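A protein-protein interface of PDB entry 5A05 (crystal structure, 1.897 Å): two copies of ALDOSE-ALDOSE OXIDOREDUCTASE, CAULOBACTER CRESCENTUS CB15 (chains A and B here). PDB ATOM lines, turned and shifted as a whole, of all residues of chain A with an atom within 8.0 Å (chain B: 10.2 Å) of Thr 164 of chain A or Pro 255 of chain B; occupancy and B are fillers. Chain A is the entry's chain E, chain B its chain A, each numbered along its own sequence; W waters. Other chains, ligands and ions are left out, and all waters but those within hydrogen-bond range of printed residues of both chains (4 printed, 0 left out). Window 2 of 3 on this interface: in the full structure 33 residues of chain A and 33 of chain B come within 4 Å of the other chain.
Hydrophobic or aromatic side chains of chain A within 4 Å of the printed part of chain B: Val 245.
Hydrophobic or aromatic side chains of chain B within 4 Å of the printed part of chain A: Pro 255 and Trp 258.
Among the printed residues, 8 pairs touch across the chains.
The backbone carbonyl oxygen of Ser 253 of chain B sits at hydrogen-bond distance from the backbone NH of Arg 155 of chain B (2.9 Å).
N of Gln 275 of chain B lies within hydrogen-bond range of O of Trp 258 of chain B.
The backbone NH (N) of Phe 163 of chain A lies within hydrogen-bond range of the backbone carbonyl oxygen (O) of Val 245 of chain A, at 3.0 Å.
OD1 of Asn 246 of chain A is in hydrogen-bond range of N of Thr 164 of chain A.
OD1 of Asp 223 of chain A sits at hydrogen-bond distance from N of Tyr 243 of chain A (2.8 Å).
The side-chain carboxylate (OD2) of Asp 223 of chain A sits at hydrogen-bond distance from the side-chain hydroxyl (OG) of Ser 244 of chain A.
No position is printed for both chains.
The guanidinium group of Arg 155 of chain B lies within salt-bridge range of the side-chain carboxylate of Asp 223 of chain A (2.8 Å).
The guanidinium group of Arg 155 of chain B sits at hydrogen-bond distance from the side-chain hydroxyl of Ser 244 of chain A, 3.0 Å away.
NE1 of Trp 258 of chain B sits close to O of Asn 246 of chain A (3.4 Å).
Among the printed residues, merely in contact across the chains: Thr 164 of chain A with Pro 255 of chain B (3.8 Å), Ser 244 of chain A with Pro 255 of chain B (3.3 Å), Val 245 of chain A with Arg 155 of chain B (3.6 Å), Val 245 of chain A with Ser 253 of chain B (3.9 Å) and Val 245 of chain A with Gly 254 of chain B (3.7 Å).
Of chain B, only Pro 255 (3.8 Å) comes within 4 Å of Thr 164 of chain A.
Ile 186 of chain A touches none of the printed residues of chain B.
Of the printed residues of chain B, Asp 223 of chain A touches Arg 155 (2.8 Å).
Of the printed residues of chain B, Val 245 of chain A touches Arg 155, Ser 253 and Gly 254.
Printed residues of chain B within 4 Å of Asn 246 of chain A: Trp 258.
Printed residues of chain A within 4 Å of Arg 155 of chain B: Asp 223 (2.8 Å), Ser 244 (3.0 Å) and Val 245 (3.6 Å).
Gly 254 of chain B touches one residue of chain A.
Of the printed residues of chain A, Pro 255 of chain B touches Thr 164 (3.8 Å) and Ser 244 (3.3 Å).
Of the printed residues of chain A, Trp 258 of chain B touches Asn 246 (3.3 Å).
Water W3 bridges OD2 of Asp 223 of chain A (2.6 Å) and NH2 of Arg 155 of chain B (3.2 Å).
Water W2 bridges OE1 of Gln 275 of chain B (2.7 Å) and ND2 of Asn 246 of chain A (2.8 Å).
Water W4 bridges OG of Ser 253 of chain B (2.8 Å) and O of Asn 246 of chain A (2.8 Å).
Water W1 lies within hydrogen-bond range of the backbone carbonyl oxygen of Gly 254 of chain B (2.8 Å) and the backbone NH of Asn 246 of chain A (2.9 Å).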
ATOM      1  N   GLY A 162       2.753  17.752  -2.060  1.00  0.00           N
ATOM      2  CA  GLY A 162       3.977  17.045  -2.358  1.00  0.00           C
ATOM      3  C   GLY A 162       4.866  17.874  -3.232  1.00  0.00           C
ATOM      4  O   GLY A 162       4.393  18.785  -3.906  1.00  0.00           O
ATOM      5  N   PHE A 163       6.160  17.576  -3.220  1.00  0.00           N
ATOM      6  CA  PHE A 163       7.023  18.126  -4.257  1.00  0.00           C
ATOM      7  C   PHE A 163       8.076  17.096  -4.605  1.00  0.00           C
ATOM      8  O   PHE A 163       8.327  16.178  -3.834  1.00  0.00           O
ATOM      9  CB  PHE A 163       7.647  19.459  -3.826  1.00  0.00           C
ATOM     10  CG  PHE A 163       8.635  19.354  -2.685  1.00  0.00           C
ATOM     11  CD1 PHE A 163       8.199  19.273  -1.373  1.00  0.00           C
ATOM     12  CD2 PHE A 163      10.000  19.382  -2.927  1.00  0.00           C
ATOM     13  CE1 PHE A 163       9.115  19.203  -0.319  1.00  0.00           C
ATOM     14  CE2 PHE A 163      10.918  19.313  -1.882  1.00  0.00           C
ATOM     15  CZ  PHE A 163      10.473  19.226  -0.581  1.00  0.00           C
ATOM     16  N   THR A 164       8.650  17.215  -5.795  1.00  0.00           N
ATOM     17  CA  THR A 164       9.708  16.315  -6.219  1.00  0.00           C
ATOM     18  C   THR A 164      11.013  16.773  -5.573  1.00  0.00           C
ATOM     19  O   THR A 164      11.666  17.690  -6.069  1.00  0.00           O
ATOM     20  CB  THR A 164       9.849  16.299  -7.750  1.00  0.00           C
ATOM     21  OG1 THR A 164       9.980  17.645  -8.216  1.00  0.00           O
ATOM     22  CG2 THR A 164       8.613  15.679  -8.396  1.00  0.00           C
ATOM     23  N   ILE A 165      11.385  16.148  -4.465  1.00  0.00           N
ATOM     24  CA  ILE A 165      12.562  16.593  -3.708  1.00  0.00           C
ATOM     25  C   ILE A 165      13.846  16.213  -4.463  1.00  0.00           C
ATOM     26  O   ILE A 165      13.867  15.235  -5.206  1.00  0.00           O
ATOM     27  CB  ILE A 165      12.555  16.012  -2.268  1.00  0.00           C
ATOM     28  CG1 ILE A 165      13.506  16.811  -1.352  1.00  0.00           C
ATOM     29  CG2 ILE A 165      12.841  14.510  -2.283  1.00  0.00           C
ATOM     30  CD1 ILE A 165      13.282  16.560   0.145  1.00  0.00           C
ATOM     31  N   GLY A 166      14.904  17.003  -4.295  1.00  0.00           N
ATOM     32  CA  GLY A 166      16.107  16.810  -5.089  1.00  0.00           C
ATOM     33  C   GLY A 166      17.270  16.101  -4.415  1.00  0.00           C
ATOM     34  O   GLY A 166      17.302  14.869  -4.302  1.00  0.00           O
ATOM     35  N   ASP A 167      18.237  16.902  -3.985  1.00  0.00           N
ATOM     36  CA  ASP A 167      19.501  16.430  -3.414  1.00  0.00           C
ATOM     37  C   ASP A 167      19.326  15.473  -2.236  1.00  0.00           C
ATOM     38  O   ASP A 167      18.821  15.870  -1.187  1.00  0.00           O
ATOM     39  CB  ASP A 167      20.323  17.653  -2.986  1.00  0.00           C
ATOM     40  CG  ASP A 167      21.666  17.286  -2.364  1.00  0.00           C
ATOM     41  OD1 ASP A 167      22.124  16.128  -2.496  1.00  0.00           O
ATOM     42  OD2 ASP A 167      22.265  18.187  -1.746  1.00  0.00           O
ATOM     43  N   GLN A 170      20.450  16.415   1.571  1.00  0.00           N
ATOM     44  CA  GLN A 170      19.873  17.504   2.360  1.00  0.00           C
ATOM     45  C   GLN A 170      19.241  16.977   3.646  1.00  0.00           C
ATOM     46  O   GLN A 170      18.885  15.804   3.724  1.00  0.00           O
ATOM     47  CB  GLN A 170      18.841  18.265   1.539  1.00  0.00           C
ATOM     48  CG  GLN A 170      17.619  17.435   1.168  1.00  0.00           C
ATOM     49  CD  GLN A 170      16.717  18.188   0.209  1.00  0.00           C
ATOM     50  OE1 GLN A 170      16.706  17.914  -0.997  1.00  0.00           O
ATOM     51  NE2 GLN A 170      15.978  19.157   0.733  1.00  0.00           N
ATOM     52  N   ILE A 186       5.796  18.257   4.184  1.00  0.00           N
ATOM     53  CA  ILE A 186       4.839  18.806   3.222  1.00  0.00           C
ATOM     54  C   ILE A 186       3.454  18.179   3.422  1.00  0.00           C
ATOM     55  O   ILE A 186       2.436  18.848   3.288  1.00  0.00           O
ATOM     56  CB  ILE A 186       5.357  18.626   1.744  1.00  0.00           C
ATOM     57  CG1 ILE A 186       4.435  19.309   0.736  1.00  0.00           C
ATOM     58  CG2 ILE A 186       5.600  17.158   1.376  1.00  0.00           C
ATOM     59  CD1 ILE A 186       4.364  20.811   0.899  1.00  0.00           C
ATOM     60  N   ASP A 215      15.841   4.157  -4.462  1.00  0.00           N
ATOM     61  CA  ASP A 215      16.023   5.554  -4.837  1.00  0.00           C
ATOM     62  C   ASP A 215      17.010   6.194  -3.862  1.00  0.00           C
ATOM     63  O   ASP A 215      16.849   6.068  -2.648  1.00  0.00           O
ATOM     64  CB  ASP A 215      14.669   6.283  -4.829  1.00  0.00           C
ATOM     65  CG  ASP A 215      14.724   7.683  -5.435  1.00  0.00           C
ATOM     66  OD1 ASP A 215      15.610   8.487  -5.071  1.00  0.00           O
ATOM     67  OD2 ASP A 215      13.836   7.994  -6.254  1.00  0.00           O
ATOM     68  N   ARG A 217      17.302   9.006  -2.790  1.00  0.00           N
ATOM     69  CA  ARG A 217      16.708   9.988  -1.891  1.00  0.00           C
ATOM     70  C   ARG A 217      16.121   9.353  -0.622  1.00  0.00           C
ATOM     71  O   ARG A 217      16.019  10.007   0.411  1.00  0.00           O
ATOM     72  CB  ARG A 217      15.610  10.778  -2.618  1.00  0.00           C
ATOM     73  CG  ARG A 217      16.122  11.656  -3.758  1.00  0.00           C
ATOM     74  CD  ARG A 217      14.956  12.232  -4.556  1.00  0.00           C
ATOM     75  NE  ARG A 217      14.244  11.205  -5.309  1.00  0.00           N
ATOM     76  CZ  ARG A 217      13.085  11.409  -5.937  1.00  0.00           C
ATOM     77  NH1 ARG A 217      12.501  12.600  -5.881  1.00  0.00           N
ATOM     78  NH2 ARG A 217      12.504  10.427  -6.612  1.00  0.00           N
ATOM     79  N   PHE A 218      15.734   8.087  -0.713  1.00  0.00           N
ATOM     80  CA  PHE A 218      14.816   7.504   0.264  1.00  0.00           C
ATOM     81  C   PHE A 218      15.390   6.319   1.045  1.00  0.00           C
ATOM     82  O   PHE A 218      14.693   5.335   1.320  1.00  0.00           O
ATOM     83  CB  PHE A 218      13.528   7.093  -0.455  1.00  0.00           C
ATOM     84  CG  PHE A 218      12.865   8.237  -1.185  1.00  0.00           C
ATOM     85  CD1 PHE A 218      12.621   9.440  -0.535  1.00  0.00           C
ATOM     86  CD2 PHE A 218      12.535   8.130  -2.527  1.00  0.00           C
ATOM     87  CE1 PHE A 218      12.032  10.513  -1.207  1.00  0.00           C
ATOM     88  CE2 PHE A 218      11.944   9.196  -3.203  1.00  0.00           C
ATOM     89  CZ  PHE A 218      11.698  10.385  -2.546  1.00  0.00           C
ATOM     90  N   ASP A 223       8.698   8.377   1.150  1.00  0.00           N
ATOM     91  CA  ASP A 223       8.343   9.184  -0.009  1.00  0.00           C
ATOM     92  C   ASP A 223       6.853   9.504   0.040  1.00  0.00           C
ATOM     93  O   ASP A 223       6.451  10.602   0.399  1.00  0.00           O
ATOM     94  CB  ASP A 223       8.701   8.436  -1.292  1.00  0.00           C
ATOM     95  CG  ASP A 223       8.167   9.119  -2.559  1.00  0.00           C
ATOM     96  OD1 ASP A 223       7.773  10.310  -2.522  1.00  0.00           O
ATOM     97  OD2 ASP A 223       8.155   8.439  -3.606  1.00  0.00           O
ATOM     98  N   ALA A 242       3.664  13.519  -0.410  1.00  0.00           N
ATOM     99  CA  ALA A 242       4.623  12.907  -1.333  1.00  0.00           C
ATOM    100  C   ALA A 242       5.934  13.679  -1.497  1.00  0.00           C
ATOM    101  O   ALA A 242       5.958  14.900  -1.425  1.00  0.00           O
ATOM    102  CB  ALA A 242       3.963  12.714  -2.705  1.00  0.00           C
ATOM    103  N   TYR A 243       7.020  12.942  -1.732  1.00  0.00           N
ATOM    104  CA  TYR A 243       8.308  13.532  -2.096  1.00  0.00           C
ATOM    105  C   TYR A 243       8.691  13.198  -3.554  1.00  0.00           C
ATOM    106  O   TYR A 243       9.787  13.545  -4.013  1.00  0.00           O
ATOM    107  CB  TYR A 243       9.407  13.033  -1.144  1.00  0.00           C
ATOM    108  CG  TYR A 243       9.724  13.926   0.049  1.00  0.00           C
ATOM    109  CD1 TYR A 243       9.341  15.263   0.079  1.00  0.00           C
ATOM    110  CD2 TYR A 243      10.436  13.424   1.132  1.00  0.00           C
ATOM    111  CE1 TYR A 243       9.655  16.076   1.168  1.00  0.00           C
ATOM    112  CE2 TYR A 243      10.765  14.224   2.213  1.00  0.00           C
ATOM    113  CZ  TYR A 243      10.376  15.543   2.229  1.00  0.00           C
ATOM    114  OH  TYR A 243      10.707  16.333   3.315  1.00  0.00           O
ATOM    115  N   SER A 244       7.808  12.523  -4.285  1.00  0.00           N
ATOM    116  CA  SER A 244       8.127  12.203  -5.676  1.00  0.00           C
ATOM    117  C   SER A 244       7.095  12.703  -6.709  1.00  0.00           C
ATOM    118  O   SER A 244       7.188  12.356  -7.884  1.00  0.00           O
ATOM    119  CB  SER A 244       8.330  10.686  -5.845  1.00  0.00           C
ATOM    120  OG  SER A 244       7.152   9.945  -5.577  1.00  0.00           O
ATOM    121  N   VAL A 245       6.113  13.494  -6.278  1.00  0.00           N
ATOM    122  CA  VAL A 245       5.230  14.187  -7.221  1.00  0.00           C
ATOM    123  C   VAL A 245       4.994  15.598  -6.743  1.00  0.00           C
ATOM    124  O   VAL A 245       5.202  15.908  -5.570  1.00  0.00           O
ATOM    125  CB  VAL A 245       3.840  13.508  -7.410  1.00  0.00           C
ATOM    126  CG1 VAL A 245       3.965  12.144  -8.042  1.00  0.00           C
ATOM    127  CG2 VAL A 245       3.060  13.444  -6.092  1.00  0.00           C
ATOM    128  N   ASN A 246       4.537  16.450  -7.656  1.00  0.00           N
ATOM    129  CA  ASN A 246       4.176  17.805  -7.311  1.00  0.00           C
ATOM    130  C   ASN A 246       2.659  17.973  -7.213  1.00  0.00           C
ATOM    131  O   ASN A 246       1.928  17.699  -8.162  1.00  0.00           O
ATOM    132  CB  ASN A 246       4.747  18.790  -8.337  1.00  0.00           C
ATOM    133  CG  ASN A 246       6.262  18.846  -8.306  1.00  0.00           C
ATOM    134  OD1 ASN A 246       6.861  19.239  -7.296  1.00  0.00           O
ATOM    135  ND2 ASN A 246       6.894  18.452  -9.412  1.00  0.00           N
ATOM    136  N   CYS A 247       2.203  18.411  -6.049  1.00  0.00           N
ATOM    137  CA  CYS A 247       0.802  18.758  -5.830  1.00  0.00           C
ATOM    138  C   CYS A 247       0.693  19.719  -4.655  1.00  0.00           C
ATOM    139  O   CYS A 247       1.496  19.674  -3.716  1.00  0.00           O
ATOM    140  CB  CYS A 247      -0.053  17.508  -5.581  1.00  0.00           C
ATOM    141  SG  CYS A 247       0.668  16.326  -4.408  1.00  0.00           S
ATOM    142  N   VAL B 146      -0.073   8.481 -19.871  1.00  0.00           N
ATOM    143  CA  VAL B 146       0.557   7.566 -18.918  1.00  0.00           C
ATOM    144  C   VAL B 146       1.371   6.509 -19.643  1.00  0.00           C
ATOM    145  O   VAL B 146       2.557   6.328 -19.356  1.00  0.00           O
ATOM    146  CB  VAL B 146      -0.482   6.870 -18.028  1.00  0.00           C
ATOM    147  CG1 VAL B 146       0.169   5.767 -17.209  1.00  0.00           C
ATOM    148  CG2 VAL B 146      -1.171   7.898 -17.129  1.00  0.00           C
ATOM    149  N   GLY B 149       4.593   7.396 -21.207  1.00  0.00           N
ATOM    150  CA  GLY B 149       5.645   7.752 -20.272  1.00  0.00           C
ATOM    151  C   GLY B 149       5.771   9.234 -19.978  1.00  0.00           C
ATOM    152  O   GLY B 149       6.772   9.671 -19.424  1.00  0.00           O
ATOM    153  N   ALA B 150       4.754  10.018 -20.324  1.00  0.00           N
ATOM    154  CA  ALA B 150       4.834  11.466 -20.143  1.00  0.00           C
ATOM    155  C   ALA B 150       4.953  11.871 -18.671  1.00  0.00           C
ATOM    156  O   ALA B 150       5.482  12.941 -18.352  1.00  0.00           O
ATOM    157  CB  ALA B 150       3.609  12.141 -20.780  1.00  0.00           C
ATOM    158  N   LEU B 151       4.461  11.012 -17.780  1.00  0.00           N
ATOM    159  CA  LEU B 151       4.427  11.304 -16.349  1.00  0.00           C
ATOM    160  C   LEU B 151       5.576  10.648 -15.609  1.00  0.00           C
ATOM    161  O   LEU B 151       5.825  10.964 -14.448  1.00  0.00           O
ATOM    162  CB  LEU B 151       3.110  10.810 -15.712  1.00  0.00           C
ATOM    163  CG  LEU B 151       1.783  11.215 -16.364  1.00  0.00           C
ATOM    164  CD1 LEU B 151       0.597  10.874 -15.445  1.00  0.00           C
ATOM    165  CD2 LEU B 151       1.807  12.684 -16.672  1.00  0.00           C
ATOM    166  N   GLY B 152       6.246   9.709 -16.273  1.00  0.00           N
ATOM    167  CA  GLY B 152       7.126   8.783 -15.581  1.00  0.00           C
ATOM    168  C   GLY B 152       6.252   7.706 -14.952  1.00  0.00           C
ATOM    169  O   GLY B 152       5.059   7.622 -15.246  1.00  0.00           O
ATOM    170  N   PRO B 153       6.830   6.886 -14.067  1.00  0.00           N
ATOM    171  CA  PRO B 153       6.016   5.867 -13.387  1.00  0.00           C
ATOM    172  C   PRO B 153       4.862   6.502 -12.608  1.00  0.00           C
ATOM    173  O   PRO B 153       5.051   7.554 -11.992  1.00  0.00           O
ATOM    174  CB  PRO B 153       7.016   5.186 -12.444  1.00  0.00           C
ATOM    175  CG  PRO B 153       8.102   6.216 -12.240  1.00  0.00           C
ATOM    176  CD  PRO B 153       8.210   6.947 -13.552  1.00  0.00           C
ATOM    177  N   VAL B 154       3.677   5.901 -12.656  1.00  0.00           N
ATOM    178  CA  VAL B 154       2.558   6.460 -11.912  1.00  0.00           C
ATOM    179  C   VAL B 154       2.822   6.314 -10.422  1.00  0.00           C
ATOM    180  O   VAL B 154       3.150   5.222  -9.946  1.00  0.00           O
ATOM    181  CB  VAL B 154       1.210   5.776 -12.244  1.00  0.00           C
ATOM    182  CG1 VAL B 154       0.130   6.273 -11.284  1.00  0.00           C
ATOM    183  CG2 VAL B 154       0.810   6.047 -13.684  1.00  0.00           C
ATOM    184  N   ARG B 155       2.667   7.409  -9.687  1.00  0.00           N
ATOM    185  CA  ARG B 155       2.891   7.406  -8.250  1.00  0.00           C
ATOM    186  C   ARG B 155       1.580   7.559  -7.486  1.00  0.00           C
ATOM    187  O   ARG B 155       1.363   6.865  -6.500  1.00  0.00           O
ATOM    188  CB  ARG B 155       3.853   8.518  -7.848  1.00  0.00           C
ATOM    189  CG  ARG B 155       5.224   8.415  -8.534  1.00  0.00           C
ATOM    190  CD  ARG B 155       5.994   7.162  -8.062  1.00  0.00           C
ATOM    191  NE  ARG B 155       6.306   7.217  -6.638  1.00  0.00           N
ATOM    192  CZ  ARG B 155       6.290   6.166  -5.820  1.00  0.00           C
ATOM    193  NH1 ARG B 155       5.972   4.961  -6.284  1.00  0.00           N
ATOM    194  NH2 ARG B 155       6.595   6.314  -4.535  1.00  0.00           N
ATOM    195  N   THR B 156       0.724   8.485  -7.926  1.00  0.00           N
ATOM    196  CA  THR B 156      -0.569   8.666  -7.276  1.00  0.00           C
ATOM    197  C   THR B 156      -1.691   8.844  -8.275  1.00  0.00           C
ATOM    198  O   THR B 156      -1.500   9.410  -9.355  1.00  0.00           O
ATOM    199  CB  THR B 156      -0.598   9.892  -6.337  1.00  0.00           C
ATOM    200  OG1 THR B 156      -0.412  11.089  -7.106  1.00  0.00           O
ATOM    201  CG2 THR B 156       0.481   9.802  -5.259  1.00  0.00           C
ATOM    202  N   ALA B 235       2.556   2.322  -7.149  1.00  0.00           N
ATOM    203  CA  ALA B 235       1.542   3.345  -7.372  1.00  0.00           C
ATOM    204  C   ALA B 235       0.473   3.266  -6.291  1.00  0.00           C
ATOM    205  O   ALA B 235       0.159   2.185  -5.794  1.00  0.00           O
ATOM    206  CB  ALA B 235       0.908   3.191  -8.747  1.00  0.00           C
ATOM    207  N   VAL B 252      -3.923  11.893 -12.237  1.00  0.00           N
ATOM    208  CA  VAL B 252      -2.871  10.894 -12.114  1.00  0.00           C
ATOM    209  C   VAL B 252      -1.515  11.618 -12.203  1.00  0.00           C
ATOM    210  O   VAL B 252      -1.318  12.493 -13.058  1.00  0.00           O
ATOM    211  CB  VAL B 252      -3.015   9.778 -13.194  1.00  0.00           C
ATOM    212  CG1 VAL B 252      -3.196  10.372 -14.566  1.00  0.00           C
ATOM    213  CG2 VAL B 252      -1.812   8.828 -13.161  1.00  0.00           C
ATOM    214  N   SER B 253      -0.604  11.296 -11.281  1.00  0.00           N
ATOM    215  CA  SER B 253       0.654  12.038 -11.149  1.00  0.00           C
ATOM    216  C   SER B 253       1.866  11.101 -11.104  1.00  0.00           C
ATOM    217  O   SER B 253       1.802  10.024 -10.513  1.00  0.00           O
ATOM    218  CB  SER B 253       0.645  12.905  -9.878  1.00  0.00           C
ATOM    219  OG  SER B 253      -0.553  13.675  -9.759  1.00  0.00           O
ATOM    220  N   GLY B 254       2.962  11.531 -11.729  1.00  0.00           N
ATOM    221  CA  GLY B 254       4.250  10.860 -11.622  1.00  0.00           C
ATOM    222  C   GLY B 254       5.343  11.913 -11.457  1.00  0.00           C
ATOM    223  O   GLY B 254       5.058  13.100 -11.443  1.00  0.00           O
ATOM    224  N   PRO B 255       6.609  11.479 -11.361  1.00  0.00           N
ATOM    225  CA  PRO B 255       7.750  12.382 -11.152  1.00  0.00           C
ATOM    226  C   PRO B 255       7.893  13.434 -12.260  1.00  0.00           C
ATOM    227  O   PRO B 255       8.442  14.495 -12.001  1.00  0.00           O
ATOM    228  CB  PRO B 255       8.973  11.451 -11.168  1.00  0.00           C
ATOM    229  CG  PRO B 255       8.478  10.084 -11.180  1.00  0.00           C
ATOM    230  CD  PRO B 255       7.021  10.083 -11.571  1.00  0.00           C
ATOM    231  N   LYS B 256       7.410  13.149 -13.466  1.00  0.00           N
ATOM    232  CA  LYS B 256       7.572  14.110 -14.568  1.00  0.00           C
ATOM    233  C   LYS B 256       6.394  15.074 -14.709  1.00  0.00           C
ATOM    234  O   LYS B 256       6.467  16.051 -15.455  1.00  0.00           O
ATOM    235  CB  LYS B 256       7.789  13.376 -15.890  1.00  0.00           C
ATOM    236  CG  LYS B 256       9.082  12.566 -15.942  1.00  0.00           C
ATOM    237  CD  LYS B 256       9.111  11.636 -17.158  1.00  0.00           C
ATOM    238  CE  LYS B 256       9.218  12.425 -18.451  1.00  0.00           C
ATOM    239  NZ  LYS B 256       9.108  11.522 -19.628  1.00  0.00           N
ATOM    240  N   GLY B 257       5.299  14.810 -14.006  1.00  0.00           N
ATOM    241  CA  GLY B 257       4.163  15.707 -14.090  1.00  0.00           C
ATOM    242  C   GLY B 257       2.840  14.998 -13.899  1.00  0.00           C
ATOM    243  O   GLY B 257       2.803  13.854 -13.460  1.00  0.00           O
ATOM    244  N   TRP B 258       1.743  15.673 -14.225  1.00  0.00           N
ATOM    245  CA  TRP B 258       0.435  15.075 -13.977  1.00  0.00           C
ATOM    246  C   TRP B 258      -0.599  15.536 -14.984  1.00  0.00           C
ATOM    247  O   TRP B 258      -0.388  16.518 -15.710  1.00  0.00           O
ATOM    248  CB  TRP B 258      -0.047  15.388 -12.545  1.00  0.00           C
ATOM    249  CG  TRP B 258      -0.083  16.863 -12.102  1.00  0.00           C
ATOM    250  CD1 TRP B 258       0.810  17.480 -11.258  1.00  0.00           C
ATOM    251  CD2 TRP B 258      -1.088  17.858 -12.404  1.00  0.00           C
ATOM    252  NE1 TRP B 258       0.436  18.785 -11.041  1.00  0.00           N
ATOM    253  CE2 TRP B 258      -0.723  19.045 -11.722  1.00  0.00           C
ATOM    254  CE3 TRP B 258      -2.252  17.864 -13.185  1.00  0.00           C
ATOM    255  CZ2 TRP B 258      -1.467  20.235 -11.816  1.00  0.00           C
ATOM    256  CZ3 TRP B 258      -2.996  19.049 -13.275  1.00  0.00           C
ATOM    257  CH2 TRP B 258      -2.601  20.213 -12.590  1.00  0.00           C
ATOM    258  N   VAL B 259      -1.706  14.802 -15.034  1.00  0.00           N
ATOM    259  CA  VAL B 259      -2.824  15.155 -15.893  1.00  0.00           C
ATOM    260  C   VAL B 259      -4.115  14.874 -15.134  1.00  0.00           C
ATOM    261  O   VAL B 259      -4.224  13.873 -14.420  1.00  0.00           O
ATOM    262  CB  VAL B 259      -2.765  14.382 -17.248  1.00  0.00           C
ATOM    263  CG1 VAL B 259      -2.681  12.901 -17.029  1.00  0.00           C
ATOM    264  CG2 VAL B 259      -3.941  14.728 -18.141  1.00  0.00           C
ATOM    265  N   GLN B 275       0.079  19.267 -16.113  1.00  0.00           N
ATOM    266  CA  GLN B 275       1.283  19.937 -15.688  1.00  0.00           C
ATOM    267  C   GLN B 275       2.424  19.061 -16.184  1.00  0.00           C
ATOM    268  O   GLN B 275       2.759  18.043 -15.576  1.00  0.00           O
ATOM    269  CB  GLN B 275       1.294  20.130 -14.165  1.00  0.00           C
ATOM    270  CG  GLN B 275       2.401  21.037 -13.634  1.00  0.00           C
ATOM    271  CD  GLN B 275       3.708  20.299 -13.498  1.00  0.00           C
ATOM    272  OE1 GLN B 275       3.864  19.451 -12.613  1.00  0.00           O
ATOM    273  NE2 GLN B 275       4.656  20.594 -14.389  1.00  0.00           N
ATOM    274  N   LEU B 276       2.975  19.429 -17.332  1.00  0.00           N
ATOM    275  CA  LEU B 276       4.029  18.650 -17.976  1.00  0.00           C
ATOM    276  C   LEU B 276       5.115  19.627 -18.396  1.00  0.00           C
ATOM    277  O   LEU B 276       4.887  20.465 -19.278  1.00  0.00           O
ATOM    278  CB  LEU B 276       3.488  17.890 -19.199  1.00  0.00           C
ATOM    279  CG  LEU B 276       2.254  16.999 -18.998  1.00  0.00           C
ATOM    280  CD1 LEU B 276       1.648  16.567 -20.324  1.00  0.00           C
ATOM    281  CD2 LEU B 276       2.615  15.800 -18.161  1.00  0.00           C
ATOM    282  N   GLY B 277       6.267  19.570 -17.748  1.00  0.00           N
ATOM    283  CA  GLY B 277       7.362  20.458 -18.091  1.00  0.00           C
ATOM    284  C   GLY B 277       7.215  21.863 -17.537  1.00  0.00           C
ATOM    285  O   GLY B 277       8.107  22.362 -16.860  1.00  0.00           O
ATOM    286  N   GLY B 278       6.089  22.507 -17.822  1.00  0.00           N
ATOM    287  CA  GLY B 278       5.833  23.837 -17.310  1.00  0.00           C
ATOM    288  C   GLY B 278       4.635  23.860 -16.385  1.00  0.00           C
ATOM    289  O   GLY B 278       4.146  22.812 -15.974  1.00  0.00           O
HETATM  290  O   HOH W   1       4.219  15.601 -10.420  1.00  0.00           O
HETATM  291  O   HOH W   2       5.692  17.611 -11.843  1.00  0.00           O
HETATM  292  O   HOH W   3       9.774   6.401  -3.963  1.00  0.00           O
HETATM  293  O   HOH W   4      -0.383  16.083  -8.326  1.00  0.00           O
